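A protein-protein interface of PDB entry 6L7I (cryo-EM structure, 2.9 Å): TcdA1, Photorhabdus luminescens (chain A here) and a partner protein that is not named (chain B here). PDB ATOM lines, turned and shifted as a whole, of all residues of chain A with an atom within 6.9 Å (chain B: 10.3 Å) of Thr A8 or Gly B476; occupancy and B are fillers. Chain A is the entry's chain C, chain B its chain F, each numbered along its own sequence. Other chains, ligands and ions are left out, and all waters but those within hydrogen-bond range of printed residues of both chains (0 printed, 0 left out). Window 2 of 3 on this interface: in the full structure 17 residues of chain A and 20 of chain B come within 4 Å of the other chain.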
ATOM      1  N   GLU A   6      -1.552 -36.544 -11.933  1.00  0.00           N
ATOM      2  CA  GLU A   6      -2.690 -35.729 -12.335  1.00  0.00           C
ATOM      3  C   GLU A   6      -3.223 -36.229 -13.668  1.00  0.00           C
ATOM      4  O   GLU A   6      -2.457 -36.413 -14.617  1.00  0.00           O
ATOM      5  CB  GLU A   6      -2.317 -34.251 -12.439  1.00  0.00           C
ATOM      6  CG  GLU A   6      -3.437 -33.396 -13.005  1.00  0.00           C
ATOM      7  CD  GLU A   6      -3.255 -31.918 -12.743  1.00  0.00           C
ATOM      8  OE1 GLU A   6      -2.500 -31.561 -11.817  1.00  0.00           O
ATOM      9  OE2 GLU A   6      -3.872 -31.113 -13.470  1.00  0.00           O
ATOM     10  N   ARG A   7      -4.530 -36.456 -13.730  1.00  0.00           N
ATOM     11  CA  ARG A   7      -5.201 -36.985 -14.906  1.00  0.00           C
ATOM     12  C   ARG A   7      -6.290 -36.021 -15.346  1.00  0.00           C
ATOM     13  O   ARG A   7      -7.077 -35.547 -14.526  1.00  0.00           O
ATOM     14  CB  ARG A   7      -5.807 -38.349 -14.607  1.00  0.00           C
ATOM     15  CG  ARG A   7      -6.547 -38.988 -15.746  1.00  0.00           C
ATOM     16  CD  ARG A   7      -5.591 -39.489 -16.795  1.00  0.00           C
ATOM     17  NE  ARG A   7      -6.142 -40.631 -17.511  1.00  0.00           N
ATOM     18  CZ  ARG A   7      -6.912 -40.541 -18.586  1.00  0.00           C
ATOM     19  NH1 ARG A   7      -7.227 -39.356 -19.084  1.00  0.00           N
ATOM     20  NH2 ARG A   7      -7.367 -41.640 -19.163  1.00  0.00           N
ATOM     21  N   THR A   8      -6.328 -35.731 -16.639  1.00  0.00           N
ATOM     22  CA  THR A   8      -7.324 -34.845 -17.219  1.00  0.00           C
ATOM     23  C   THR A   8      -8.268 -35.655 -18.090  1.00  0.00           C
ATOM     24  O   THR A   8      -7.831 -36.332 -19.024  1.00  0.00           O
ATOM     25  CB  THR A   8      -6.663 -33.740 -18.038  1.00  0.00           C
ATOM     26  OG1 THR A   8      -5.847 -32.938 -17.180  1.00  0.00           O
ATOM     27  CG2 THR A   8      -7.702 -32.866 -18.671  1.00  0.00           C
ATOM     28  N   VAL A   9      -9.558 -35.591 -17.779  1.00  0.00           N
ATOM     29  CA  VAL A   9     -10.590 -36.331 -18.489  1.00  0.00           C
ATOM     30  C   VAL A   9     -11.541 -35.328 -19.118  1.00  0.00           C
ATOM     31  O   VAL A   9     -12.126 -34.500 -18.414  1.00  0.00           O
ATOM     32  CB  VAL A   9     -11.345 -37.286 -17.556  1.00  0.00           C
ATOM     33  CG1 VAL A   9     -12.467 -37.959 -18.288  1.00  0.00           C
ATOM     34  CG2 VAL A   9     -10.402 -38.321 -17.006  1.00  0.00           C
ATOM     35  N   SER A  10     -11.697 -35.399 -20.432  1.00  0.00           N
ATOM     36  CA  SER A  10     -12.694 -34.598 -21.130  1.00  0.00           C
ATOM     37  C   SER A  10     -13.962 -35.421 -21.288  1.00  0.00           C
ATOM     38  O   SER A  10     -13.920 -36.528 -21.828  1.00  0.00           O
ATOM     39  CB  SER A  10     -12.179 -34.152 -22.494  1.00  0.00           C
ATOM     40  OG  SER A  10     -13.255 -33.766 -23.323  1.00  0.00           O
ATOM     41  N   GLU A  13     -14.949 -36.388 -24.905  1.00  0.00           N
ATOM     42  CA  GLU A  13     -14.206 -37.506 -25.468  1.00  0.00           C
ATOM     43  C   GLU A  13     -14.607 -38.829 -24.840  1.00  0.00           C
ATOM     44  O   GLU A  13     -14.364 -39.881 -25.434  1.00  0.00           O
ATOM     45  CB  GLU A  13     -12.704 -37.295 -25.298  1.00  0.00           C
ATOM     46  CG  GLU A  13     -12.150 -36.117 -26.080  1.00  0.00           C
ATOM     47  CD  GLU A  13     -10.645 -35.982 -25.941  1.00  0.00           C
ATOM     48  OE1 GLU A  13     -10.057 -36.713 -25.119  1.00  0.00           O
ATOM     49  OE2 GLU A  13     -10.048 -35.160 -26.667  1.00  0.00           O
ATOM     50  N   THR A  92     -13.081 -27.836 -14.612  1.00  0.00           N
ATOM     51  CA  THR A  92     -13.097 -26.595 -15.380  1.00  0.00           C
ATOM     52  C   THR A  92     -14.176 -26.667 -16.447  1.00  0.00           C
ATOM     53  O   THR A  92     -14.208 -27.614 -17.235  1.00  0.00           O
ATOM     54  CB  THR A  92     -11.740 -26.336 -16.041  1.00  0.00           C
ATOM     55  OG1 THR A  92     -10.760 -26.064 -15.037  1.00  0.00           O
ATOM     56  CG2 THR A  92     -11.797 -25.166 -16.987  1.00  0.00           C
ATOM     57  N   ASN A 129     -10.196 -24.507 -12.903  1.00  0.00           N
ATOM     58  CA  ASN A 129      -9.530 -25.488 -12.039  1.00  0.00           C
ATOM     59  C   ASN A 129     -10.199 -25.529 -10.669  1.00  0.00           C
ATOM     60  O   ASN A 129      -9.549 -25.512  -9.624  1.00  0.00           O
ATOM     61  CB  ASN A 129      -8.030 -25.203 -11.928  1.00  0.00           C
ATOM     62  CG  ASN A 129      -7.223 -26.429 -11.554  1.00  0.00           C
ATOM     63  OD1 ASN A 129      -7.624 -27.557 -11.825  1.00  0.00           O
ATOM     64  ND2 ASN A 129      -6.074 -26.211 -10.928  1.00  0.00           N
ATOM     65  N   ILE A 182     -14.492 -30.670 -18.311  1.00  0.00           N
ATOM     66  CA  ILE A 182     -13.125 -31.129 -18.090  1.00  0.00           C
ATOM     67  C   ILE A 182     -12.969 -31.440 -16.612  1.00  0.00           C
ATOM     68  O   ILE A 182     -13.224 -30.575 -15.771  1.00  0.00           O
ATOM     69  CB  ILE A 182     -12.096 -30.072 -18.518  1.00  0.00           C
ATOM     70  CG1 ILE A 182     -12.498 -29.406 -19.833  1.00  0.00           C
ATOM     71  CG2 ILE A 182     -10.728 -30.688 -18.640  1.00  0.00           C
ATOM     72  CD1 ILE A 182     -12.546 -30.329 -21.008  1.00  0.00           C
ATOM     73  N   LEU A 183     -12.540 -32.653 -16.291  1.00  0.00           N
ATOM     74  CA  LEU A 183     -12.251 -33.038 -14.916  1.00  0.00           C
ATOM     75  C   LEU A 183     -10.751 -33.210 -14.752  1.00  0.00           C
ATOM     76  O   LEU A 183     -10.114 -33.895 -15.554  1.00  0.00           O
ATOM     77  CB  LEU A 183     -12.955 -34.339 -14.530  1.00  0.00           C
ATOM     78  CG  LEU A 183     -14.463 -34.481 -14.690  1.00  0.00           C
ATOM     79  CD1 LEU A 183     -14.861 -35.874 -14.292  1.00  0.00           C
ATOM     80  CD2 LEU A 183     -15.201 -33.473 -13.859  1.00  0.00           C
ATOM     81  N   HIS A 184     -10.193 -32.595 -13.718  1.00  0.00           N
ATOM     82  CA  HIS A 184      -8.785 -32.766 -13.372  1.00  0.00           C
ATOM     83  C   HIS A 184      -8.727 -33.705 -12.175  1.00  0.00           C
ATOM     84  O   HIS A 184      -8.944 -33.304 -11.035  1.00  0.00           O
ATOM     85  CB  HIS A 184      -8.126 -31.431 -13.068  1.00  0.00           C
ATOM     86  CG  HIS A 184      -8.566 -30.323 -13.967  1.00  0.00           C
ATOM     87  ND1 HIS A 184      -8.085 -30.168 -15.247  1.00  0.00           N
ATOM     88  CD2 HIS A 184      -9.441 -29.312 -13.769  1.00  0.00           C
ATOM     89  CE1 HIS A 184      -8.650 -29.111 -15.799  1.00  0.00           C
ATOM     90  NE2 HIS A 184      -9.477 -28.575 -14.924  1.00  0.00           N
ATOM     91  N   ILE A 185      -8.437 -34.971 -12.444  1.00  0.00           N
ATOM     92  CA  ILE A 185      -8.350 -35.988 -11.407  1.00  0.00           C
ATOM     93  C   ILE A 185      -6.908 -36.076 -10.935  1.00  0.00           C
ATOM     94  O   ILE A 185      -6.005 -36.376 -11.720  1.00  0.00           O
ATOM     95  CB  ILE A 185      -8.842 -37.346 -11.922  1.00  0.00           C
ATOM     96  CG1 ILE A 185     -10.302 -37.253 -12.340  1.00  0.00           C
ATOM     97  CG2 ILE A 185      -8.669 -38.408 -10.864  1.00  0.00           C
ATOM     98  CD1 ILE A 185     -10.727 -38.347 -13.261  1.00  0.00           C
ATOM     99  N   VAL B 453     -13.365 -18.234 -18.392  1.00  0.00           N
ATOM    100  CA  VAL B 453     -12.155 -18.798 -17.810  1.00  0.00           C
ATOM    101  C   VAL B 453     -11.122 -17.685 -17.790  1.00  0.00           C
ATOM    102  O   VAL B 453     -10.396 -17.477 -18.765  1.00  0.00           O
ATOM    103  CB  VAL B 453     -11.645 -20.022 -18.587  1.00  0.00           C
ATOM    104  CG1 VAL B 453     -10.609 -20.755 -17.772  1.00  0.00           C
ATOM    105  CG2 VAL B 453     -12.780 -20.952 -18.933  1.00  0.00           C
ATOM    106  N   ASP B 455      -8.475 -17.246 -15.843  1.00  0.00           N
ATOM    107  CA  ASP B 455      -7.167 -17.590 -15.310  1.00  0.00           C
ATOM    108  C   ASP B 455      -6.303 -18.193 -16.403  1.00  0.00           C
ATOM    109  O   ASP B 455      -6.798 -18.963 -17.233  1.00  0.00           O
ATOM    110  CB  ASP B 455      -7.288 -18.578 -14.149  1.00  0.00           C
ATOM    111  CG  ASP B 455      -7.629 -17.902 -12.835  1.00  0.00           C
ATOM    112  OD1 ASP B 455      -7.894 -16.681 -12.830  1.00  0.00           O
ATOM    113  OD2 ASP B 455      -7.634 -18.600 -11.800  1.00  0.00           O
ATOM    114  N   ASN B 456      -5.012 -17.838 -16.379  1.00  0.00           N
ATOM    115  CA  ASN B 456      -3.994 -18.308 -17.326  1.00  0.00           C
ATOM    116  C   ASN B 456      -4.385 -18.007 -18.772  1.00  0.00           C
ATOM    117  O   ASN B 456      -4.420 -18.892 -19.626  1.00  0.00           O
ATOM    118  CB  ASN B 456      -3.699 -19.800 -17.147  1.00  0.00           C
ATOM    119  CG  ASN B 456      -3.502 -20.189 -15.704  1.00  0.00           C
ATOM    120  OD1 ASN B 456      -2.401 -20.092 -15.172  1.00  0.00           O
ATOM    121  ND2 ASN B 456      -4.566 -20.650 -15.067  1.00  0.00           N
ATOM    122  N   ILE B 472      -6.678 -19.475 -23.554  1.00  0.00           N
ATOM    123  CA  ILE B 472      -6.592 -20.031 -22.211  1.00  0.00           C
ATOM    124  C   ILE B 472      -5.651 -21.223 -22.258  1.00  0.00           C
ATOM    125  O   ILE B 472      -6.013 -22.280 -22.770  1.00  0.00           O
ATOM    126  CB  ILE B 472      -7.970 -20.445 -21.686  1.00  0.00           C
ATOM    127  CG1 ILE B 472      -8.940 -19.270 -21.728  1.00  0.00           C
ATOM    128  CG2 ILE B 472      -7.851 -20.977 -20.285  1.00  0.00           C
ATOM    129  CD1 ILE B 472     -10.308 -19.644 -22.207  1.00  0.00           C
ATOM    130  N   THR B 473      -4.446 -21.066 -21.721  1.00  0.00           N
ATOM    131  CA  THR B 473      -3.508 -22.179 -21.575  1.00  0.00           C
ATOM    132  C   THR B 473      -3.366 -22.441 -20.084  1.00  0.00           C
ATOM    133  O   THR B 473      -2.410 -21.995 -19.450  1.00  0.00           O
ATOM    134  CB  THR B 473      -2.183 -21.882 -22.200  1.00  0.00           C
ATOM    135  OG1 THR B 473      -1.568 -20.794 -21.503  1.00  0.00           O
ATOM    136  CG2 THR B 473      -2.358 -21.500 -23.651  1.00  0.00           C
ATOM    137  N   GLY B 474      -4.319 -23.180 -19.531  1.00  0.00           N
ATOM    138  CA  GLY B 474      -4.321 -23.495 -18.127  1.00  0.00           C
ATOM    139  C   GLY B 474      -3.663 -24.830 -17.870  1.00  0.00           C
ATOM    140  O   GLY B 474      -3.009 -25.397 -18.750  1.00  0.00           O
ATOM    141  N   PRO B 475      -3.824 -25.360 -16.653  1.00  0.00           N
ATOM    142  CA  PRO B 475      -3.157 -26.632 -16.327  1.00  0.00           C
ATOM    143  C   PRO B 475      -3.773 -27.828 -17.026  1.00  0.00           C
ATOM    144  O   PRO B 475      -3.043 -28.726 -17.456  1.00  0.00           O
ATOM    145  CB  PRO B 475      -3.306 -26.725 -14.800  1.00  0.00           C
ATOM    146  CG  PRO B 475      -3.726 -25.352 -14.352  1.00  0.00           C
ATOM    147  CD  PRO B 475      -4.503 -24.784 -15.485  1.00  0.00           C
ATOM    148  N   GLY B 476      -5.093 -27.864 -17.163  1.00  0.00           N
ATOM    149  CA  GLY B 476      -5.744 -29.014 -17.751  1.00  0.00           C
ATOM    150  C   GLY B 476      -6.080 -28.877 -19.221  1.00  0.00           C
ATOM    151  O   GLY B 476      -5.846 -29.803 -20.000  1.00  0.00           O
ATOM    152  N   LEU B 477      -6.639 -27.736 -19.611  1.00  0.00           N
ATOM    153  CA  LEU B 477      -7.002 -27.486 -20.994  1.00  0.00           C
ATOM    154  C   LEU B 477      -6.112 -26.421 -21.608  1.00  0.00           C
ATOM    155  O   LEU B 477      -5.454 -25.645 -20.915  1.00  0.00           O
ATOM    156  CB  LEU B 477      -8.471 -27.062 -21.128  1.00  0.00           C
ATOM    157  CG  LEU B 477      -9.142 -25.988 -20.270  1.00  0.00           C
ATOM    158  CD1 LEU B 477      -8.868 -24.567 -20.706  1.00  0.00           C
ATOM    159  CD2 LEU B 477     -10.613 -26.232 -20.347  1.00  0.00           C
ATOM    160  N   ARG B 478      -6.129 -26.383 -22.934  1.00  0.00           N
ATOM    161  CA  ARG B 478      -5.472 -25.341 -23.702  1.00  0.00           C
ATOM    162  C   ARG B 478      -6.307 -25.072 -24.943  1.00  0.00           C
ATOM    163  O   ARG B 478      -6.666 -26.000 -25.668  1.00  0.00           O
ATOM    164  CB  ARG B 478      -4.039 -25.744 -24.055  1.00  0.00           C
ATOM    165  CG  ARG B 478      -3.882 -27.186 -24.458  1.00  0.00           C
ATOM    166  CD  ARG B 478      -2.477 -27.670 -24.199  1.00  0.00           C
ATOM    167  NE  ARG B 478      -2.220 -27.916 -22.788  1.00  0.00           N
ATOM    168  CZ  ARG B 478      -2.337 -29.107 -22.217  1.00  0.00           C
ATOM    169  NH1 ARG B 478      -2.707 -30.150 -22.941  1.00  0.00           N
ATOM    170  NH2 ARG B 478      -2.083 -29.257 -20.927  1.00  0.00           N
ATOM    171  N   GLY B 479      -6.638 -23.813 -25.166  1.00  0.00           N
ATOM    172  CA  GLY B 479      -7.534 -23.448 -26.241  1.00  0.00           C
ATOM    173  C   GLY B 479      -7.956 -22.003 -26.097  1.00  0.00           C
ATOM    174  O   GLY B 479      -7.487 -21.281 -25.221  1.00  0.00           O
ATOM    175  N   PHE B 492     -15.371 -22.444 -27.007  1.00  0.00           N
ATOM    176  CA  PHE B 492     -14.016 -22.903 -26.731  1.00  0.00           C
ATOM    177  C   PHE B 492     -13.499 -23.760 -27.878  1.00  0.00           C
ATOM    178  O   PHE B 492     -14.071 -24.809 -28.186  1.00  0.00           O
ATOM    179  CB  PHE B 492     -13.998 -23.683 -25.422  1.00  0.00           C
ATOM    180  CG  PHE B 492     -12.631 -24.094 -24.976  1.00  0.00           C
ATOM    181  CD1 PHE B 492     -11.757 -23.170 -24.444  1.00  0.00           C
ATOM    182  CD2 PHE B 492     -12.226 -25.408 -25.078  1.00  0.00           C
ATOM    183  CE1 PHE B 492     -10.507 -23.543 -24.032  1.00  0.00           C
ATOM    184  CE2 PHE B 492     -10.973 -25.790 -24.669  1.00  0.00           C
ATOM    185  CZ  PHE B 492     -10.115 -24.857 -24.149  1.00  0.00           C
ATOM    186  N   PRO B 494     -10.299 -25.899 -28.916  1.00  0.00           N
ATOM    187  CA  PRO B 494      -9.045 -26.419 -28.364  1.00  0.00           C
ATOM    188  C   PRO B 494      -7.912 -26.368 -29.371  1.00  0.00           C
ATOM    189  O   PRO B 494      -8.092 -26.656 -30.556  1.00  0.00           O
ATOM    190  CB  PRO B 494      -9.397 -27.865 -28.000  1.00  0.00           C
ATOM    191  CG  PRO B 494     -10.872 -27.913 -27.982  1.00  0.00           C
ATOM    192  CD  PRO B 494     -11.329 -26.942 -28.998  1.00  0.00           C
ATOM    193  N   LEU B 495      -6.734 -25.988 -28.887  1.00  0.00           N
ATOM    194  CA  LEU B 495      -5.542 -26.003 -29.720  1.00  0.00           C
ATOM    195  C   LEU B 495      -5.125 -27.439 -29.991  1.00  0.00           C
ATOM    196  O   LEU B 495      -5.123 -28.279 -29.090  1.00  0.00           O
ATOM    197  CB  LEU B 495      -4.408 -25.246 -29.041  1.00  0.00           C
ATOM    198  CG  LEU B 495      -4.677 -23.766 -28.798  1.00  0.00           C
ATOM    199  CD1 LEU B 495      -3.795 -23.248 -27.688  1.00  0.00           C
ATOM    200  CD2 LEU B 495      -4.447 -22.987 -30.058  1.00  0.00           C
ATOM    201  N   LEU B 498       0.085 -27.914 -28.392  1.00  0.00           N
ATOM    202  CA  LEU B 498       0.787 -26.841 -27.720  1.00  0.00           C
ATOM    203  C   LEU B 498       2.094 -27.381 -27.162  1.00  0.00           C
ATOM    204  O   LEU B 498       2.128 -28.506 -26.656  1.00  0.00           O
ATOM    205  CB  LEU B 498      -0.058 -26.259 -26.586  1.00  0.00           C
ATOM    206  CG  LEU B 498       0.218 -24.824 -26.162  1.00  0.00           C
ATOM    207  CD1 LEU B 498      -0.122 -23.880 -27.288  1.00  0.00           C
ATOM    208  CD2 LEU B 498      -0.569 -24.499 -24.930  1.00  0.00           C
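The side-chain hydroxyl of Thr A92 sits at hydrogen-bond distance from the backbone NH of Asn A129 (2.7 Å). O of Ile A182 is in hydrogen-bond range of N of Thr A92 (3.0 Å). The side-chain hydroxyl of Thr A92 sits at hydrogen-bond distance from a ring nitrogen (NE2) of His A184 (2.8 Å).
Thr A8 touches Gly B476 (CG2 to O, 3.8 Å). Leu B477 touches Thr A92 (CD2 to CG2, 3.7 Å). Leu B477 touches Ile A182. Gly B476 touches His A184.
Of chain A, only Thr A8 and His A184 come within 4 Å of Gly B476. No residue of chain B comes within 4 Å of Arg A7. Of the printed residues of chain B, His A184 touches Gly B476 (3.5 Å). Printed residues of chain B within 4 Å of Ile A182: Leu B477 (3.7 Å). The nearest residue of chain B that does not touch Thr A8 is Pro B475 (5.1 Å). The nearest residue of chain A that does not touch Gly B476 is Ile A182 (5.0 Å).
Of the 12 printed residues of chain A, 4 touch a printed residue of chain B. Hydrophobic or aromatic side chains of chain A that line the printed part of chain B: Ile A182 and His A184. Printed residues of chain B that touch a printed residue of chain A: Gly B476 and Leu B477. Hydrophobic or aromatic side chains of chain B within 4 Å of the printed part of chain A: Leu B477.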
